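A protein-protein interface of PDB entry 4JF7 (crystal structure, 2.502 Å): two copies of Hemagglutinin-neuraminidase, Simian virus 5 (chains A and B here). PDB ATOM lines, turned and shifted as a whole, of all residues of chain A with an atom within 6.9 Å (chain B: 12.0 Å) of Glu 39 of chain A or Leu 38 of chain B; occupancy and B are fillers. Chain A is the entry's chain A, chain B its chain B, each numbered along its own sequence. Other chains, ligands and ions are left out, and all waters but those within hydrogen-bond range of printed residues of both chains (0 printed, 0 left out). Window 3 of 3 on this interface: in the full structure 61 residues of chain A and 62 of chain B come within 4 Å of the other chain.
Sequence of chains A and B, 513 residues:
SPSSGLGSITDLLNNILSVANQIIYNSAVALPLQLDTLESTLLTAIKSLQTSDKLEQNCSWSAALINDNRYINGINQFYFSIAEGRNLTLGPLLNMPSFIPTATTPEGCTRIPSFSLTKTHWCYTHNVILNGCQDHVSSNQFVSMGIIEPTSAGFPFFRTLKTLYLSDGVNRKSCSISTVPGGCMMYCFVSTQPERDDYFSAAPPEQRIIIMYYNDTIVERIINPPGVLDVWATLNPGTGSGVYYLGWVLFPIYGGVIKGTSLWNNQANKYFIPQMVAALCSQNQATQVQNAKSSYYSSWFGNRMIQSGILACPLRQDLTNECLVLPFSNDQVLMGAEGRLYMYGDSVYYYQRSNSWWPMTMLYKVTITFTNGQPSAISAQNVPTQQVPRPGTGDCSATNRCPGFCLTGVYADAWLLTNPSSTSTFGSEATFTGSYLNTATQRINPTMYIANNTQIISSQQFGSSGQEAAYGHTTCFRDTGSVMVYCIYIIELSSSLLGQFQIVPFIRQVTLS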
ATOM      1  N   GLN A  34     -16.351  37.955 -19.619  1.00  0.00           N
ATOM      2  CA  GLN A  34     -14.902  37.891 -19.538  1.00  0.00           C
ATOM      3  C   GLN A  34     -14.451  36.432 -19.579  1.00  0.00           C
ATOM      4  O   GLN A  34     -13.324  36.130 -19.977  1.00  0.00           O
ATOM      5  CB  GLN A  34     -14.404  38.569 -18.264  1.00  0.00           C
ATOM      6  CG  GLN A  34     -12.901  38.773 -18.230  1.00  0.00           C
ATOM      7  CD  GLN A  34     -12.413  39.262 -16.886  1.00  0.00           C
ATOM      8  OE1 GLN A  34     -13.152  39.240 -15.901  1.00  0.00           O
ATOM      9  NE2 GLN A  34     -11.161  39.709 -16.836  1.00  0.00           N
ATOM     10  N   LEU A  35     -15.345  35.531 -19.173  1.00  0.00           N
ATOM     11  CA  LEU A  35     -15.092  34.094 -19.254  1.00  0.00           C
ATOM     12  C   LEU A  35     -15.168  33.572 -20.691  1.00  0.00           C
ATOM     13  O   LEU A  35     -14.410  32.680 -21.075  1.00  0.00           O
ATOM     14  CB  LEU A  35     -16.057  33.310 -18.357  1.00  0.00           C
ATOM     15  CG  LEU A  35     -15.783  33.316 -16.851  1.00  0.00           C
ATOM     16  CD1 LEU A  35     -16.754  32.404 -16.120  1.00  0.00           C
ATOM     17  CD2 LEU A  35     -14.348  32.901 -16.567  1.00  0.00           C
ATOM     18  N   ASP A  36     -16.084  34.119 -21.484  1.00  0.00           N
ATOM     19  CA  ASP A  36     -16.187  33.721 -22.883  1.00  0.00           C
ATOM     20  C   ASP A  36     -15.008  34.258 -23.682  1.00  0.00           C
ATOM     21  O   ASP A  36     -14.423  33.540 -24.497  1.00  0.00           O
ATOM     22  CB  ASP A  36     -17.504  34.195 -23.495  1.00  0.00           C
ATOM     23  CG  ASP A  36     -18.704  33.511 -22.882  1.00  0.00           C
ATOM     24  OD1 ASP A  36     -18.530  32.412 -22.308  1.00  0.00           O
ATOM     25  OD2 ASP A  36     -19.817  34.074 -22.974  1.00  0.00           O
ATOM     26  N   THR A  37     -14.669  35.522 -23.446  1.00  0.00           N
ATOM     27  CA  THR A  37     -13.504  36.139 -24.074  1.00  0.00           C
ATOM     28  C   THR A  37     -12.220  35.361 -23.752  1.00  0.00           C
ATOM     29  O   THR A  37     -11.400  35.113 -24.639  1.00  0.00           O
ATOM     30  CB  THR A  37     -13.341  37.607 -23.631  1.00  0.00           C
ATOM     31  OG1 THR A  37     -14.475  38.368 -24.068  1.00  0.00           O
ATOM     32  CG2 THR A  37     -12.065  38.213 -24.211  1.00  0.00           C
ATOM     33  N   LEU A  38     -12.063  34.976 -22.484  1.00  0.00           N
ATOM     34  CA  LEU A  38     -10.920  34.177 -22.024  1.00  0.00           C
ATOM     35  C   LEU A  38     -10.814  32.842 -22.767  1.00  0.00           C
ATOM     36  O   LEU A  38      -9.758  32.518 -23.314  1.00  0.00           O
ATOM     37  CB  LEU A  38     -10.996  33.939 -20.507  1.00  0.00           C
ATOM     38  CG  LEU A  38      -9.881  33.150 -19.806  1.00  0.00           C
ATOM     39  CD1 LEU A  38      -9.712  33.615 -18.377  1.00  0.00           C
ATOM     40  CD2 LEU A  38     -10.192  31.678 -19.800  1.00  0.00           C
ATOM     41  N   GLU A  39     -11.907  32.075 -22.766  1.00  0.00           N
ATOM     42  CA  GLU A  39     -11.967  30.760 -23.414  1.00  0.00           C
ATOM     43  C   GLU A  39     -11.564  30.813 -24.885  1.00  0.00           C
ATOM     44  O   GLU A  39     -10.826  29.953 -25.371  1.00  0.00           O
ATOM     45  CB  GLU A  39     -13.383  30.174 -23.291  1.00  0.00           C
ATOM     46  CG  GLU A  39     -13.532  28.726 -23.775  1.00  0.00           C
ATOM     47  CD  GLU A  39     -14.958  28.194 -23.640  1.00  0.00           C
ATOM     48  OE1 GLU A  39     -15.909  29.005 -23.626  1.00  0.00           O
ATOM     49  OE2 GLU A  39     -15.130  26.960 -23.546  1.00  0.00           O
ATOM     50  N   SER A  40     -12.060  31.827 -25.584  1.00  0.00           N
ATOM     51  CA  SER A  40     -11.780  31.996 -27.001  1.00  0.00           C
ATOM     52  C   SER A  40     -10.303  32.280 -27.272  1.00  0.00           C
ATOM     53  O   SER A  40      -9.730  31.718 -28.202  1.00  0.00           O
ATOM     54  CB  SER A  40     -12.641  33.118 -27.583  1.00  0.00           C
ATOM     55  OG  SER A  40     -12.293  34.367 -27.013  1.00  0.00           O
ATOM     56  N   THR A  41      -9.688  33.141 -26.462  1.00  0.00           N
ATOM     57  CA  THR A  41      -8.301  33.544 -26.701  1.00  0.00           C
ATOM     58  C   THR A  41      -7.297  32.415 -26.483  1.00  0.00           C
ATOM     59  O   THR A  41      -6.186  32.459 -27.020  1.00  0.00           O
ATOM     60  CB  THR A  41      -7.866  34.742 -25.829  1.00  0.00           C
ATOM     61  OG1 THR A  41      -7.866  34.357 -24.449  1.00  0.00           O
ATOM     62  CG2 THR A  41      -8.781  35.941 -26.038  1.00  0.00           C
ATOM     63  N   LEU A  42      -7.668  31.410 -25.694  1.00  0.00           N
ATOM     64  CA  LEU A  42      -6.748  30.298 -25.464  1.00  0.00           C
ATOM     65  C   LEU A  42      -7.128  29.003 -26.187  1.00  0.00           C
ATOM     66  O   LEU A  42      -6.294  28.114 -26.350  1.00  0.00           O
ATOM     67  CB  LEU A  42      -6.471  30.074 -23.973  1.00  0.00           C
ATOM     68  CG  LEU A  42      -7.597  29.902 -22.958  1.00  0.00           C
ATOM     69  CD1 LEU A  42      -8.320  28.590 -23.177  1.00  0.00           C
ATOM     70  CD2 LEU A  42      -7.019  29.980 -21.555  1.00  0.00           C
ATOM     71  N   LEU A  43      -8.381  28.895 -26.618  1.00  0.00           N
ATOM     72  CA  LEU A  43      -8.748  27.855 -27.570  1.00  0.00           C
ATOM     73  C   LEU A  43      -8.067  28.190 -28.892  1.00  0.00           C
ATOM     74  O   LEU A  43      -7.723  27.300 -29.668  1.00  0.00           O
ATOM     75  CB  LEU A  43     -10.268  27.769 -27.750  1.00  0.00           C
ATOM     76  CG  LEU A  43     -11.052  26.812 -26.846  1.00  0.00           C
ATOM     77  CD1 LEU A  43     -12.546  27.033 -27.003  1.00  0.00           C
ATOM     78  CD2 LEU A  43     -10.701  25.370 -27.160  1.00  0.00           C
ATOM     79  N   THR A  44      -7.871  29.488 -29.126  1.00  0.00           N
ATOM     80  CA  THR A  44      -7.152  29.996 -30.296  1.00  0.00           C
ATOM     81  C   THR A  44      -5.680  30.201 -29.948  1.00  0.00           C
ATOM     82  O   THR A  44      -5.086  31.243 -30.236  1.00  0.00           O
ATOM     83  CB  THR A  44      -7.747  31.334 -30.795  1.00  0.00           C
ATOM     84  OG1 THR A  44      -9.174  31.313 -30.655  1.00  0.00           O
ATOM     85  CG2 THR A  44      -7.384  31.580 -32.258  1.00  0.00           C
ATOM     86  N   VAL B  29     -24.050  28.768  -8.224  1.00  0.00           N
ATOM     87  CA  VAL B  29     -24.570  27.809  -9.200  1.00  0.00           C
ATOM     88  C   VAL B  29     -24.154  28.152 -10.637  1.00  0.00           C
ATOM     89  O   VAL B  29     -23.489  27.356 -11.308  1.00  0.00           O
ATOM     90  CB  VAL B  29     -26.115  27.703  -9.117  1.00  0.00           C
ATOM     91  CG1 VAL B  29     -26.616  26.495  -9.899  1.00  0.00           C
ATOM     92  CG2 VAL B  29     -26.566  27.622  -7.667  1.00  0.00           C
ATOM     93  N   ALA B  30     -24.544  29.345 -11.087  1.00  0.00           N
ATOM     94  CA  ALA B  30     -24.333  29.801 -12.464  1.00  0.00           C
ATOM     95  C   ALA B  30     -22.864  29.848 -12.892  1.00  0.00           C
ATOM     96  O   ALA B  30     -22.514  29.414 -13.993  1.00  0.00           O
ATOM     97  CB  ALA B  30     -24.989  31.170 -12.671  1.00  0.00           C
ATOM     98  N   LEU B  31     -22.011  30.383 -12.026  1.00  0.00           N
ATOM     99  CA  LEU B  31     -20.587  30.502 -12.337  1.00  0.00           C
ATOM    100  C   LEU B  31     -19.776  29.200 -12.172  1.00  0.00           C
ATOM    101  O   LEU B  31     -18.958  28.882 -13.036  1.00  0.00           O
ATOM    102  CB  LEU B  31     -19.949  31.678 -11.580  1.00  0.00           C
ATOM    103  CG  LEU B  31     -20.465  33.060 -11.994  1.00  0.00           C
ATOM    104  CD1 LEU B  31     -19.807  34.165 -11.179  1.00  0.00           C
ATOM    105  CD2 LEU B  31     -20.263  33.289 -13.484  1.00  0.00           C
ATOM    106  N   PRO B  32     -19.988  28.448 -11.071  1.00  0.00           N
ATOM    107  CA  PRO B  32     -19.289  27.157 -10.982  1.00  0.00           C
ATOM    108  C   PRO B  32     -19.704  26.153 -12.065  1.00  0.00           C
ATOM    109  O   PRO B  32     -18.907  25.292 -12.437  1.00  0.00           O
ATOM    110  CB  PRO B  32     -19.693  26.640  -9.598  1.00  0.00           C
ATOM    111  CG  PRO B  32     -19.954  27.868  -8.813  1.00  0.00           C
ATOM    112  CD  PRO B  32     -20.606  28.811  -9.782  1.00  0.00           C
ATOM    113  N   LEU B  33     -20.934  26.261 -12.556  1.00  0.00           N
ATOM    114  CA  LEU B  33     -21.386  25.398 -13.638  1.00  0.00           C
ATOM    115  C   LEU B  33     -20.665  25.761 -14.933  1.00  0.00           C
ATOM    116  O   LEU B  33     -20.269  24.886 -15.707  1.00  0.00           O
ATOM    117  CB  LEU B  33     -22.899  25.514 -13.829  1.00  0.00           C
ATOM    118  CG  LEU B  33     -23.476  24.665 -14.961  1.00  0.00           C
ATOM    119  CD1 LEU B  33     -23.221  23.182 -14.707  1.00  0.00           C
ATOM    120  CD2 LEU B  33     -24.960  24.944 -15.143  1.00  0.00           C
ATOM    121  N   GLN B  34     -20.493  27.060 -15.156  1.00  0.00           N
ATOM    122  CA  GLN B  34     -19.843  27.556 -16.362  1.00  0.00           C
ATOM    123  C   GLN B  34     -18.354  27.242 -16.361  1.00  0.00           C
ATOM    124  O   GLN B  34     -17.807  26.808 -17.377  1.00  0.00           O
ATOM    125  CB  GLN B  34     -20.057  29.064 -16.508  1.00  0.00           C
ATOM    126  CG  GLN B  34     -19.329  29.680 -17.690  1.00  0.00           C
ATOM    127  CD  GLN B  34     -19.663  31.147 -17.885  1.00  0.00           C
ATOM    128  OE1 GLN B  34     -20.497  31.714 -17.169  1.00  0.00           O
ATOM    129  NE2 GLN B  34     -19.014  31.772 -18.862  1.00  0.00           N
ATOM    130  N   LEU B  35     -17.705  27.466 -15.219  1.00  0.00           N
ATOM    131  CA  LEU B  35     -16.282  27.176 -15.073  1.00  0.00           C
ATOM    132  C   LEU B  35     -16.000  25.696 -15.294  1.00  0.00           C
ATOM    133  O   LEU B  35     -14.957  25.328 -15.831  1.00  0.00           O
ATOM    134  CB  LEU B  35     -15.779  27.613 -13.694  1.00  0.00           C
ATOM    135  CG  LEU B  35     -15.693  29.120 -13.430  1.00  0.00           C
ATOM    136  CD1 LEU B  35     -15.520  29.399 -11.945  1.00  0.00           C
ATOM    137  CD2 LEU B  35     -14.555  29.735 -14.226  1.00  0.00           C
ATOM    138  N   ASP B  36     -16.938  24.851 -14.881  1.00  0.00           N
ATOM    139  CA  ASP B  36     -16.823  23.410 -15.083  1.00  0.00           C
ATOM    140  C   ASP B  36     -16.955  23.014 -16.556  1.00  0.00           C
ATOM    141  O   ASP B  36     -16.206  22.168 -17.053  1.00  0.00           O
ATOM    142  CB  ASP B  36     -17.873  22.674 -14.249  1.00  0.00           C
ATOM    143  CG  ASP B  36     -17.478  22.553 -12.796  1.00  0.00           C
ATOM    144  OD1 ASP B  36     -16.689  23.396 -12.321  1.00  0.00           O
ATOM    145  OD2 ASP B  36     -17.954  21.610 -12.130  1.00  0.00           O
ATOM    146  N   THR B  37     -17.916  23.622 -17.245  1.00  0.00           N
ATOM    147  CA  THR B  37     -18.165  23.318 -18.649  1.00  0.00           C
ATOM    148  C   THR B  37     -16.999  23.821 -19.481  1.00  0.00           C
ATOM    149  O   THR B  37     -16.508  23.125 -20.373  1.00  0.00           O
ATOM    150  CB  THR B  37     -19.461  23.989 -19.143  1.00  0.00           C
ATOM    151  OG1 THR B  37     -20.390  24.093 -18.057  1.00  0.00           O
ATOM    152  CG2 THR B  37     -20.086  23.188 -20.277  1.00  0.00           C
ATOM    153  N   LEU B  38     -16.561  25.036 -19.164  1.00  0.00           N
ATOM    154  CA  LEU B  38     -15.444  25.686 -19.841  1.00  0.00           C
ATOM    155  C   LEU B  38     -14.139  24.902 -19.696  1.00  0.00           C
ATOM    156  O   LEU B  38     -13.284  24.916 -20.587  1.00  0.00           O
ATOM    157  CB  LEU B  38     -15.272  27.108 -19.302  1.00  0.00           C
ATOM    158  CG  LEU B  38     -13.912  27.786 -19.442  1.00  0.00           C
ATOM    159  CD1 LEU B  38     -14.100  29.199 -19.937  1.00  0.00           C
ATOM    160  CD2 LEU B  38     -13.191  27.784 -18.107  1.00  0.00           C
ATOM    161  N   GLU B  39     -13.996  24.223 -18.565  1.00  0.00           N
ATOM    162  CA  GLU B  39     -12.842  23.371 -18.336  1.00  0.00           C
ATOM    163  C   GLU B  39     -12.838  22.191 -19.305  1.00  0.00           C
ATOM    164  O   GLU B  39     -11.795  21.826 -19.848  1.00  0.00           O
ATOM    165  CB  GLU B  39     -12.842  22.866 -16.897  1.00  0.00           C
ATOM    166  CG  GLU B  39     -11.745  21.866 -16.608  1.00  0.00           C
ATOM    167  CD  GLU B  39     -11.733  21.422 -15.166  1.00  0.00           C
ATOM    168  OE1 GLU B  39     -10.981  20.475 -14.850  1.00  0.00           O
ATOM    169  OE2 GLU B  39     -12.472  22.019 -14.352  1.00  0.00           O
ATOM    170  N   SER B  40     -14.013  21.604 -19.519  1.00  0.00           N
ATOM    171  CA  SER B  40     -14.159  20.445 -20.396  1.00  0.00           C
ATOM    172  C   SER B  40     -13.827  20.778 -21.855  1.00  0.00           C
ATOM    173  O   SER B  40     -13.243  19.961 -22.571  1.00  0.00           O
ATOM    174  CB  SER B  40     -15.578  19.875 -20.285  1.00  0.00           C
ATOM    175  OG  SER B  40     -15.702  18.647 -20.984  1.00  0.00           O
ATOM    176  N   THR B  41     -14.202  21.982 -22.285  1.00  0.00           N
ATOM    177  CA  THR B  41     -13.972  22.432 -23.657  1.00  0.00           C
ATOM    178  C   THR B  41     -12.484  22.532 -23.948  1.00  0.00           C
ATOM    179  O   THR B  41     -12.009  22.157 -25.025  1.00  0.00           O
ATOM    180  CB  THR B  41     -14.615  23.812 -23.901  1.00  0.00           C
ATOM    181  OG1 THR B  41     -16.027  23.733 -23.666  1.00  0.00           O
ATOM    182  CG2 THR B  41     -14.361  24.283 -25.330  1.00  0.00           C
ATOM    183  N   LEU B  42     -11.757  23.044 -22.964  1.00  0.00           N
ATOM    184  CA  LEU B  42     -10.319  23.225 -23.074  1.00  0.00           C
ATOM    185  C   LEU B  42      -9.598  21.879 -23.067  1.00  0.00           C
ATOM    186  O   LEU B  42      -8.675  21.661 -23.849  1.00  0.00           O
ATOM    187  CB  LEU B  42      -9.813  24.116 -21.937  1.00  0.00           C
ATOM    188  CG  LEU B  42      -9.880  25.635 -22.141  1.00  0.00           C
ATOM    189  CD1 LEU B  42     -11.112  26.080 -22.919  1.00  0.00           C
ATOM    190  CD2 LEU B  42      -9.819  26.347 -20.802  1.00  0.00           C
ATOM    191  N   LEU B  43     -10.037  20.981 -22.191  1.00  0.00           N
ATOM    192  CA  LEU B  43      -9.469  19.638 -22.104  1.00  0.00           C
ATOM    193  C   LEU B  43      -9.817  18.774 -23.323  1.00  0.00           C
ATOM    194  O   LEU B  43      -9.001  17.968 -23.765  1.00  0.00           O
ATOM    195  CB  LEU B  43      -9.904  18.955 -20.804  1.00  0.00           C
ATOM    196  CG  LEU B  43      -9.318  19.535 -19.514  1.00  0.00           C
ATOM    197  CD1 LEU B  43     -10.165  19.154 -18.303  1.00  0.00           C
ATOM    198  CD2 LEU B  43      -7.872  19.080 -19.324  1.00  0.00           C
ATOM    199  N   THR B  44     -11.023  18.941 -23.861  1.00  0.00           N
ATOM    200  CA  THR B  44     -11.393  18.283 -25.113  1.00  0.00           C
ATOM    201  C   THR B  44     -10.454  18.729 -26.232  1.00  0.00           C
ATOM    202  O   THR B  44      -9.987  17.913 -27.027  1.00  0.00           O
ATOM    203  CB  THR B  44     -12.858  18.584 -25.514  1.00  0.00           C
ATOM    204  OG1 THR B  44     -13.743  18.044 -24.525  1.00  0.00           O
ATOM    205  CG2 THR B  44     -13.197  17.973 -26.878  1.00  0.00           C
ATOM    206  N   ALA B  45     -10.168  20.026 -26.276  1.00  0.00           N
ATOM    207  CA  ALA B  45      -9.265  20.579 -27.281  1.00  0.00           C
ATOM    208  C   ALA B  45      -7.798  20.187 -27.042  1.00  0.00           C
ATOM    209  O   ALA B  45      -7.018  20.077 -27.990  1.00  0.00           O
ATOM    210  CB  ALA B  45      -9.411  22.091 -27.345  1.00  0.00           C
ATOM    211  N   ILE B  46      -7.430  19.989 -25.778  1.00  0.00           N
ATOM    212  CA  ILE B  46      -6.074  19.563 -25.422  1.00  0.00           C
ATOM    213  C   ILE B  46      -5.886  18.088 -25.753  1.00  0.00           C
ATOM    214  O   ILE B  46      -4.869  17.695 -26.318  1.00  0.00           O
ATOM    215  CB  ILE B  46      -5.771  19.777 -23.918  1.00  0.00           C
ATOM    216  CG1 ILE B  46      -5.645  21.268 -23.593  1.00  0.00           C
ATOM    217  CG2 ILE B  46      -4.495  19.053 -23.519  1.00  0.00           C
ATOM    218  CD1 ILE B  46      -5.801  21.592 -22.112  1.00  0.00           C
ATOM    219  N   LYS B  47      -6.879  17.281 -25.389  1.00  0.00           N
ATOM    220  CA  LYS B  47      -6.885  15.862 -25.711  1.00  0.00           C
ATOM    221  C   LYS B  47      -6.958  15.678 -27.225  1.00  0.00           C
ATOM    222  O   LYS B  47      -6.501  14.667 -27.762  1.00  0.00           O
ATOM    223  CB  LYS B  47      -8.064  15.169 -25.021  1.00  0.00           C
ATOM    224  CG  LYS B  47      -8.223  13.695 -25.362  1.00  0.00           C
ATOM    225  CD  LYS B  47      -9.359  13.049 -24.574  1.00  0.00           C
ATOM    226  CE  LYS B  47     -10.726  13.633 -24.934  1.00  0.00           C
ATOM    227  NZ  LYS B  47     -11.206  13.204 -26.280  1.00  0.00           N
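The side-chain hydroxyl (OG1) of Thr 41 of chain B lies close to the side-chain carboxylate (OE2) of Glu 39 of chain A, 3.4 Å away.
The backbone carbonyl oxygen of Asp 36 of chain A sits at hydrogen-bond distance from the side-chain hydroxyl of Ser 40 of chain A, at 3.4 Å.
O of Thr 37 of chain B is in hydrogen-bond range of OG1 of Thr 41 of chain B (3.4 Å).
Among the printed residues, pairs that only touch across the chains: Leu 35 of chain A with Gln 34 of chain B (3.4 Å), Leu 35 of chain A with Leu 35 of chain B (3.9 Å), Leu 35 of chain A with Leu 38 of chain B (3.7 Å), Asp 36 of chain A with Gln 34 of chain B (3.5 Å), Glu 39 of chain A with Leu 38 of chain B (3.6 Å), Glu 39 of chain A with Leu 42 of chain B (3.7 Å), Leu 42 of chain A with Leu 42 of chain B (3.5 Å), Leu 43 of chain A with Thr 41 of chain B (3.7 Å), Leu 43 of chain A with Leu 42 of chain B (3.995 Å) and Leu 43 of chain A with Ala 45 of chain B (3.5 Å).
Of the printed residues of chain B, Asp 36 of chain A touches Gln 34 (3.5 Å).
No residue of chain B comes within 4 Å of Thr 37 of chain A.
No residue of chain B comes within 4 Å of Leu 38 of chain A.
Glu 39 of chain A touches just these residues of chain B: Leu 38 (3.6 Å), Thr 41 (3.2 Å) and Leu 42 (3.7 Å).
No residue of chain B comes within 4 Å of Ser 40 of chain A.
No residue of chain B comes within 4 Å of Thr 41 of chain A.
Leu 42 of chain A touches one residue of chain B.
No residue of chain B comes within 4 Å of Thr 44 of chain A.
Pro 32 of chain B touches none of the printed residues of chain A.
Of the printed residues of chain A, Gln 34 of chain B touches Leu 35 (3.4 Å) and Asp 36 (3.5 Å).
Of chain A, only Leu 35 (3.7 Å) and Glu 39 (3.6 Å) come within 4 Å of Leu 38 of chain B.
Printed residues of chain A within 4 Å of Leu 42 of chain B: Glu 39 (3.7 Å), Leu 42 (3.5 Å) and Leu 43 (3.995 Å).
Of the 19 printed residues of chain B, 6 touch a printed residue of chain A.
Hydrophobic or aromatic side chains of chain B within 4 Å of the printed part of chain A: Leu 35, Leu 38, Leu 42 and Ala 45.
Leu 35 of chain A touches Gln 34 of chain B, but with the chains exchanged Gln 34 of chain A does not touch Leu 35 of chain B (8.6 Å).
Glu 39 of chain A touches Leu 38 of chain B, but with the chains exchanged Leu 38 of chain A does not touch Glu 39 of chain B (8.5 Å).
Leu 42 of chain A touches its own counterpart, Leu 42 of chain B.
Leu 43 of chain A touches Leu 42 of chain B, but with the chains exchanged Leu 42 of chain A does not touch Leu 43 of chain B (7.9 Å).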
